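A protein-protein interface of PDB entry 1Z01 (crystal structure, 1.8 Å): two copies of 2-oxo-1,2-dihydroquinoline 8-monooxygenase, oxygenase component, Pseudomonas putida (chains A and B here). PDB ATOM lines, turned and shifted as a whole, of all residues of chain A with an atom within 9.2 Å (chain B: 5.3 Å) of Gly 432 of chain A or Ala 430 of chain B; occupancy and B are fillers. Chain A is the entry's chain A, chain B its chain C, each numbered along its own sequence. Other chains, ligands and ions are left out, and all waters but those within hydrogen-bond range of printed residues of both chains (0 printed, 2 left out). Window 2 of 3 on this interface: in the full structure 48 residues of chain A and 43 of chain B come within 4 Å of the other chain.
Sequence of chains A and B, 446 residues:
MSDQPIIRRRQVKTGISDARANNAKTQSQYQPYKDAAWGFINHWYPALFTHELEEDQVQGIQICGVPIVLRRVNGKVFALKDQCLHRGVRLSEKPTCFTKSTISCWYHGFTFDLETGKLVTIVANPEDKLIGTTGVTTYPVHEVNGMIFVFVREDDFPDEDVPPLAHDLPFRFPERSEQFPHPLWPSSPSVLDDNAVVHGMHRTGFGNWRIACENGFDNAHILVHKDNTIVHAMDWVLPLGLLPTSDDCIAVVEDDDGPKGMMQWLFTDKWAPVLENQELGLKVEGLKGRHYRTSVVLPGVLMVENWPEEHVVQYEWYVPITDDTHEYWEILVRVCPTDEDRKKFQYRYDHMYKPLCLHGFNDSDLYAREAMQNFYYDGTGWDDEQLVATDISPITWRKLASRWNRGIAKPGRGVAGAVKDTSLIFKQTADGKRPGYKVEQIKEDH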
ATOM      1  N   PHE A 206     -39.452 -26.761 -22.115  1.00  0.00           N
ATOM      2  CA  PHE A 206     -38.890 -27.435 -23.263  1.00  0.00           C
ATOM      3  C   PHE A 206     -39.843 -28.441 -23.879  1.00  0.00           C
ATOM      4  O   PHE A 206     -40.082 -29.514 -23.327  1.00  0.00           O
ATOM      5  CB  PHE A 206     -37.554 -28.053 -22.860  1.00  0.00           C
ATOM      6  CG  PHE A 206     -36.651 -27.069 -22.184  1.00  0.00           C
ATOM      7  CD1 PHE A 206     -36.643 -26.956 -20.799  1.00  0.00           C
ATOM      8  CD2 PHE A 206     -35.911 -26.159 -22.937  1.00  0.00           C
ATOM      9  CE1 PHE A 206     -35.920 -25.942 -20.171  1.00  0.00           C
ATOM     10  CE2 PHE A 206     -35.187 -25.143 -22.311  1.00  0.00           C
ATOM     11  CZ  PHE A 206     -35.196 -25.036 -20.927  1.00  0.00           C
ATOM     12  N   ILE A 425     -26.421 -21.840 -32.442  1.00  0.00           N
ATOM     13  CA  ILE A 425     -27.107 -22.580 -31.382  1.00  0.00           C
ATOM     14  C   ILE A 425     -26.154 -23.592 -30.720  1.00  0.00           C
ATOM     15  O   ILE A 425     -26.192 -23.781 -29.499  1.00  0.00           O
ATOM     16  CB  ILE A 425     -28.374 -23.268 -31.934  1.00  0.00           C
ATOM     17  CG1 ILE A 425     -29.461 -22.208 -32.150  1.00  0.00           C
ATOM     18  CG2 ILE A 425     -28.868 -24.351 -30.969  1.00  0.00           C
ATOM     19  CD1 ILE A 425     -30.634 -22.695 -32.958  1.00  0.00           C
ATOM     20  N   PHE A 426     -25.277 -24.221 -31.501  1.00  0.00           N
ATOM     21  CA  PHE A 426     -24.330 -25.155 -30.902  1.00  0.00           C
ATOM     22  C   PHE A 426     -23.315 -24.413 -30.041  1.00  0.00           C
ATOM     23  O   PHE A 426     -22.881 -24.929 -29.008  1.00  0.00           O
ATOM     24  CB  PHE A 426     -23.614 -25.993 -31.970  1.00  0.00           C
ATOM     25  CG  PHE A 426     -24.431 -27.162 -32.452  1.00  0.00           C
ATOM     26  CD1 PHE A 426     -25.080 -27.120 -33.676  1.00  0.00           C
ATOM     27  CD2 PHE A 426     -24.609 -28.280 -31.635  1.00  0.00           C
ATOM     28  CE1 PHE A 426     -25.902 -28.164 -34.081  1.00  0.00           C
ATOM     29  CE2 PHE A 426     -25.431 -29.333 -32.034  1.00  0.00           C
ATOM     30  CZ  PHE A 426     -26.082 -29.271 -33.263  1.00  0.00           C
ATOM     31  N   LYS A 427     -22.947 -23.201 -30.454  1.00  0.00           N
ATOM     32  CA  LYS A 427     -21.995 -22.397 -29.690  1.00  0.00           C
ATOM     33  C   LYS A 427     -22.587 -22.089 -28.320  1.00  0.00           C
ATOM     34  O   LYS A 427     -21.942 -22.286 -27.287  1.00  0.00           O
ATOM     35  CB  LYS A 427     -21.698 -21.077 -30.409  1.00  0.00           C
ATOM     36  CG  LYS A 427     -20.929 -20.073 -29.556  1.00  0.00           C
ATOM     37  CD  LYS A 427     -20.967 -18.675 -30.147  1.00  0.00           C
ATOM     38  CE  LYS A 427     -20.252 -17.674 -29.241  1.00  0.00           C
ATOM     39  NZ  LYS A 427     -20.214 -16.275 -29.805  1.00  0.00           N
ATOM     40  N   GLN A 428     -23.824 -21.599 -28.328  1.00  0.00           N
ATOM     41  CA  GLN A 428     -24.518 -21.245 -27.107  1.00  0.00           C
ATOM     42  C   GLN A 428     -24.710 -22.456 -26.215  1.00  0.00           C
ATOM     43  O   GLN A 428     -24.563 -22.357 -25.003  1.00  0.00           O
ATOM     44  CB  GLN A 428     -25.876 -20.627 -27.433  1.00  0.00           C
ATOM     45  CG  GLN A 428     -25.783 -19.326 -28.211  1.00  0.00           C
ATOM     46  CD  GLN A 428     -27.152 -18.780 -28.602  1.00  0.00           C
ATOM     47  OE1 GLN A 428     -27.257 -17.713 -29.213  1.00  0.00           O
ATOM     48  NE2 GLN A 428     -28.206 -19.513 -28.251  1.00  0.00           N
ATOM     49  N   THR A 429     -25.041 -23.594 -26.822  1.00  0.00           N
ATOM     50  CA  THR A 429     -25.251 -24.840 -26.078  1.00  0.00           C
ATOM     51  C   THR A 429     -23.927 -25.303 -25.443  1.00  0.00           C
ATOM     52  O   THR A 429     -23.883 -25.724 -24.277  1.00  0.00           O
ATOM     53  CB  THR A 429     -25.795 -25.952 -27.012  1.00  0.00           C
ATOM     54  OG1 THR A 429     -26.963 -25.473 -27.689  1.00  0.00           O
ATOM     55  CG2 THR A 429     -26.185 -27.182 -26.213  1.00  0.00           C
ATOM     56  N   ALA A 430     -22.847 -25.211 -26.213  1.00  0.00           N
ATOM     57  CA  ALA A 430     -21.529 -25.601 -25.736  1.00  0.00           C
ATOM     58  C   ALA A 430     -21.190 -24.763 -24.517  1.00  0.00           C
ATOM     59  O   ALA A 430     -20.627 -25.268 -23.546  1.00  0.00           O
ATOM     60  CB  ALA A 430     -20.482 -25.380 -26.838  1.00  0.00           C
ATOM     61  N   ASP A 431     -21.537 -23.481 -24.563  1.00  0.00           N
ATOM     62  CA  ASP A 431     -21.261 -22.571 -23.446  1.00  0.00           C
ATOM     63  C   ASP A 431     -22.150 -22.867 -22.237  1.00  0.00           C
ATOM     64  O   ASP A 431     -21.979 -22.265 -21.176  1.00  0.00           O
ATOM     65  CB  ASP A 431     -21.448 -21.108 -23.877  1.00  0.00           C
ATOM     66  CG  ASP A 431     -20.368 -20.632 -24.835  1.00  0.00           C
ATOM     67  OD1 ASP A 431     -20.459 -19.477 -25.314  1.00  0.00           O
ATOM     68  OD2 ASP A 431     -19.428 -21.414 -25.107  1.00  0.00           O
ATOM     69  N   GLY A 432     -23.097 -23.787 -22.392  1.00  0.00           N
ATOM     70  CA  GLY A 432     -23.971 -24.136 -21.288  1.00  0.00           C
ATOM     71  C   GLY A 432     -25.324 -23.448 -21.286  1.00  0.00           C
ATOM     72  O   GLY A 432     -26.103 -23.630 -20.350  1.00  0.00           O
ATOM     73  N   LYS A 433     -25.622 -22.670 -22.324  1.00  0.00           N
ATOM     74  CA  LYS A 433     -26.902 -21.962 -22.396  1.00  0.00           C
ATOM     75  C   LYS A 433     -28.040 -22.771 -23.025  1.00  0.00           C
ATOM     76  O   LYS A 433     -27.939 -23.259 -24.147  1.00  0.00           O
ATOM     77  CB  LYS A 433     -26.721 -20.642 -23.155  1.00  0.00           C
ATOM     78  CG  LYS A 433     -25.677 -19.730 -22.527  1.00  0.00           C
ATOM     79  CD  LYS A 433     -25.382 -18.514 -23.387  1.00  0.00           C
ATOM     80  CE  LYS A 433     -24.252 -17.690 -22.789  1.00  0.00           C
ATOM     81  NZ  LYS A 433     -23.882 -16.528 -23.657  1.00  0.00           N
ATOM     82  N   ARG A 434     -29.125 -22.913 -22.278  1.00  0.00           N
ATOM     83  CA  ARG A 434     -30.298 -23.645 -22.739  1.00  0.00           C
ATOM     84  C   ARG A 434     -31.166 -22.773 -23.648  1.00  0.00           C
ATOM     85  O   ARG A 434     -31.015 -21.546 -23.683  1.00  0.00           O
ATOM     86  CB  ARG A 434     -31.169 -24.052 -21.554  1.00  0.00           C
ATOM     87  CG  ARG A 434     -30.557 -24.990 -20.546  1.00  0.00           C
ATOM     88  CD  ARG A 434     -31.518 -25.078 -19.395  1.00  0.00           C
ATOM     89  NE  ARG A 434     -31.277 -26.226 -18.539  1.00  0.00           N
ATOM     90  CZ  ARG A 434     -32.089 -26.588 -17.553  1.00  0.00           C
ATOM     91  NH1 ARG A 434     -31.807 -27.652 -16.811  1.00  0.00           N
ATOM     92  NH2 ARG A 434     -33.188 -25.882 -17.309  1.00  0.00           N
ATOM     93  N   PRO A 435     -32.093 -23.401 -24.393  1.00  0.00           N
ATOM     94  CA  PRO A 435     -32.983 -22.646 -25.282  1.00  0.00           C
ATOM     95  C   PRO A 435     -33.696 -21.651 -24.372  1.00  0.00           C
ATOM     96  O   PRO A 435     -34.049 -21.991 -23.245  1.00  0.00           O
ATOM     97  CB  PRO A 435     -33.912 -23.726 -25.824  1.00  0.00           C
ATOM     98  CG  PRO A 435     -32.996 -24.927 -25.914  1.00  0.00           C
ATOM     99  CD  PRO A 435     -32.282 -24.855 -24.571  1.00  0.00           C
ATOM    100  N   GLY A 436     -33.919 -20.430 -24.842  1.00  0.00           N
ATOM    101  CA  GLY A 436     -34.543 -19.446 -23.977  1.00  0.00           C
ATOM    102  C   GLY A 436     -35.694 -18.618 -24.504  1.00  0.00           C
ATOM    103  O   GLY A 436     -36.380 -19.005 -25.452  1.00  0.00           O
ATOM    104  N   GLU A 440     -30.515 -12.041 -24.944  1.00  0.00           N
ATOM    105  CA  GLU A 440     -29.328 -11.635 -24.194  1.00  0.00           C
ATOM    106  C   GLU A 440     -28.751 -10.407 -24.892  1.00  0.00           C
ATOM    107  O   GLU A 440     -28.651 -10.379 -26.117  1.00  0.00           O
ATOM    108  CB  GLU A 440     -28.303 -12.765 -24.218  1.00  0.00           C
ATOM    109  CG  GLU A 440     -27.446 -12.882 -22.976  1.00  0.00           C
ATOM    110  CD  GLU A 440     -26.436 -14.019 -23.076  1.00  0.00           C
ATOM    111  OE1 GLU A 440     -26.048 -14.563 -22.021  1.00  0.00           O
ATOM    112  OE2 GLU A 440     -26.026 -14.366 -24.204  1.00  0.00           O
ATOM    113  N   ILE B 425     -33.249 -32.147 -26.239  1.00  0.00           N
ATOM    114  CA  ILE B 425     -31.880 -32.622 -26.422  1.00  0.00           C
ATOM    115  C   ILE B 425     -30.903 -31.458 -26.267  1.00  0.00           C
ATOM    116  O   ILE B 425     -29.824 -31.631 -25.703  1.00  0.00           O
ATOM    117  CB  ILE B 425     -31.695 -33.295 -27.803  1.00  0.00           C
ATOM    118  CG1 ILE B 425     -32.295 -34.706 -27.762  1.00  0.00           C
ATOM    119  CG2 ILE B 425     -30.207 -33.361 -28.180  1.00  0.00           C
ATOM    120  CD1 ILE B 425     -32.509 -35.317 -29.121  1.00  0.00           C
ATOM    121  N   PHE B 426     -31.267 -30.274 -26.757  1.00  0.00           N
ATOM    122  CA  PHE B 426     -30.385 -29.129 -26.600  1.00  0.00           C
ATOM    123  C   PHE B 426     -30.297 -28.731 -25.131  1.00  0.00           C
ATOM    124  O   PHE B 426     -29.242 -28.316 -24.663  1.00  0.00           O
ATOM    125  CB  PHE B 426     -30.849 -27.940 -27.460  1.00  0.00           C
ATOM    126  CG  PHE B 426     -30.365 -28.010 -28.879  1.00  0.00           C
ATOM    127  CD1 PHE B 426     -31.242 -28.300 -29.916  1.00  0.00           C
ATOM    128  CD2 PHE B 426     -29.014 -27.857 -29.170  1.00  0.00           C
ATOM    129  CE1 PHE B 426     -30.785 -28.445 -31.228  1.00  0.00           C
ATOM    130  CE2 PHE B 426     -28.547 -28.002 -30.477  1.00  0.00           C
ATOM    131  CZ  PHE B 426     -29.438 -28.298 -31.507  1.00  0.00           C
ATOM    132  N   LYS B 427     -31.401 -28.869 -24.401  1.00  0.00           N
ATOM    133  CA  LYS B 427     -31.400 -28.545 -22.975  1.00  0.00           C
ATOM    134  C   LYS B 427     -30.447 -29.494 -22.253  1.00  0.00           C
ATOM    135  O   LYS B 427     -29.586 -29.061 -21.502  1.00  0.00           O
ATOM    136  CB  LYS B 427     -32.806 -28.696 -22.386  1.00  0.00           C
ATOM    137  CG  LYS B 427     -32.854 -28.605 -20.870  1.00  0.00           C
ATOM    138  CD  LYS B 427     -34.167 -29.161 -20.328  1.00  0.00           C
ATOM    139  CE  LYS B 427     -34.151 -29.229 -18.804  1.00  0.00           C
ATOM    140  NZ  LYS B 427     -35.439 -29.741 -18.227  1.00  0.00           N
ATOM    141  N   GLN B 428     -30.603 -30.791 -22.492  1.00  0.00           N
ATOM    142  CA  GLN B 428     -29.748 -31.785 -21.859  1.00  0.00           C
ATOM    143  C   GLN B 428     -28.289 -31.548 -22.195  1.00  0.00           C
ATOM    144  O   GLN B 428     -27.427 -31.648 -21.329  1.00  0.00           O
ATOM    145  CB  GLN B 428     -30.152 -33.191 -22.301  1.00  0.00           C
ATOM    146  CG  GLN B 428     -31.543 -33.593 -21.861  1.00  0.00           C
ATOM    147  CD  GLN B 428     -31.990 -34.918 -22.460  1.00  0.00           C
ATOM    148  OE1 GLN B 428     -33.107 -35.371 -22.213  1.00  0.00           O
ATOM    149  NE2 GLN B 428     -31.118 -35.544 -23.253  1.00  0.00           N
ATOM    150  N   THR B 429     -28.017 -31.224 -23.454  1.00  0.00           N
ATOM    151  CA  THR B 429     -26.657 -30.974 -23.918  1.00  0.00           C
ATOM    152  C   THR B 429     -26.066 -29.735 -23.250  1.00  0.00           C
ATOM    153  O   THR B 429     -24.876 -29.699 -22.897  1.00  0.00           O
ATOM    154  CB  THR B 429     -26.642 -30.783 -25.436  1.00  0.00           C
ATOM    155  OG1 THR B 429     -27.282 -31.908 -26.046  1.00  0.00           O
ATOM    156  CG2 THR B 429     -25.216 -30.668 -25.955  1.00  0.00           C
ATOM    157  N   ALA B 430     -26.899 -28.715 -23.088  1.00  0.00           N
ATOM    158  CA  ALA B 430     -26.463 -27.489 -22.441  1.00  0.00           C
ATOM    159  C   ALA B 430     -26.063 -27.803 -21.004  1.00  0.00           C
ATOM    160  O   ALA B 430     -25.117 -27.219 -20.472  1.00  0.00           O
ATOM    161  CB  ALA B 430     -27.587 -26.468 -22.463  1.00  0.00           C
ATOM    162  N   ASP B 431     -26.785 -28.730 -20.382  1.00  0.00           N
ATOM    163  CA  ASP B 431     -26.525 -29.138 -19.010  1.00  0.00           C
ATOM    164  C   ASP B 431     -25.295 -30.025 -18.883  1.00  0.00           C
ATOM    165  O   ASP B 431     -24.886 -30.374 -17.777  1.00  0.00           O
ATOM    166  CB  ASP B 431     -27.741 -29.862 -18.445  1.00  0.00           C
ATOM    167  CG  ASP B 431     -28.909 -28.930 -18.208  1.00  0.00           C
ATOM    168  OD1 ASP B 431     -29.968 -29.416 -17.760  1.00  0.00           O
ATOM    169  OD2 ASP B 431     -28.767 -27.715 -18.462  1.00  0.00           O
ATOM    170  N   GLY B 432     -24.722 -30.395 -20.023  1.00  0.00           N
ATOM    171  CA  GLY B 432     -23.525 -31.212 -20.025  1.00  0.00           C
ATOM    172  C   GLY B 432     -23.766 -32.693 -20.176  1.00  0.00           C
ATOM    173  O   GLY B 432     -22.852 -33.491 -19.997  1.00  0.00           O
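NH1 of Arg 434 of chain A is in salt-bridge range of OD1 of Asp 431 of chain B, at 2.7 Å.
The backbone carbonyl oxygen of Gln 428 of chain A lies within hydrogen-bond range of the backbone NH of Lys 433 of chain A (2.9 Å). The backbone carbonyl oxygen (O) of Ile 425 of chain A lies within hydrogen-bond range of the side-chain hydroxyl (OG1) of Thr 429 of chain A, at 2.6 Å. OE2 of Glu 440 of chain A lies within salt-bridge range of NZ of Lys 433 of chain A, at 3.1 Å. O of Ile 425 of chain B lies within hydrogen-bond range of OG1 of Thr 429 of chain B (2.6 Å).
CD1 of Phe 206 of chain A touches CD of Lys 427 of chain B, 3.3 Å away. Phe 426 of chain B touches Ile 425 of chain A (CE2 to CG2, 3.7 Å). CE2 of Phe 426 of chain A touches CE2 of Phe 426 of chain B, 3.7 Å away. Thr 429 of chain A touches Phe 426 of chain B. Thr 429 of chain B touches Thr 429 of chain A. Ala 430 of chain B touches Thr 429 of chain A. CA of Gly 432 of chain A touches O of Ala 430 of chain B (3.4 Å). Ala 430 of chain B touches Lys 433 of chain A (CB to O, 3.6 Å). NH1 of Arg 434 of chain A touches CE of Lys 427 of chain B, at 3.5 Å. Arg 434 of chain A touches Ala 430 of chain B.
Printed residues of chain B within 4 Å of Gly 432 of chain A: Ala 430 (3.4 Å). Of chain A, only Thr 429 (3.6 Å), Gly 432 (3.4 Å), Lys 433 (3.6 Å) and Arg 434 (3.8 Å) come within 4 Å of Ala 430 of chain B. Printed residues of chain A within 4 Å of Thr 429 of chain B: Thr 429. Printed residues of chain A within 4 Å of Asp 431 of chain B: Arg 434. Of the printed residues of chain B, Arg 434 of chain A touches Lys 427, Ala 430 and Asp 431. Printed residues of chain B within 4 Å of Lys 433 of chain A: Ala 430. Ile 425 of chain B touches none of the printed residues of chain A. The nearest residue of chain B that does not touch Gly 432 of chain A is Asp 431 of chain B (5.1 Å). The nearest printed residue of chain B that does not touch Ile 425 of chain A is Ala 430 of chain B (7.7 Å).
Of the 8 printed residues of chain B, 5 touch a printed residue of chain A. Hydrophobic or aromatic side chains of chain B within 4 Å of the printed part of chain A: Phe 426 and Ala 430. Hydrophobic or aromatic side chains of chain A that line the printed part of chain B: Phe 206, Ile 425 and Phe 426.
Ile 425 of chain A touches Phe 426 of chain B, but with the chains exchanged Phe 426 of chain A does not touch Ile 425 of chain B (7.3 Å). Phe 426 of chain A touches its own counterpart, Phe 426 of chain B. Thr 429 of chain A touches Phe 426 of chain B, but with the chains exchanged Phe 426 of chain A does not touch Thr 429 of chain B (6.2 Å). Thr 429 of chain A touches Ala 430 of chain B, but with the chains exchanged Ala 430 of chain A does not touch Thr 429 of chain B (5.9 Å). Positions printed for both chains: 425, 426, 427, 428, 429, 430, 431 and 432. Of the 11 pairs that touch across the chains among the printed residues, 2 have their exchanged pair printed and touching as well.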
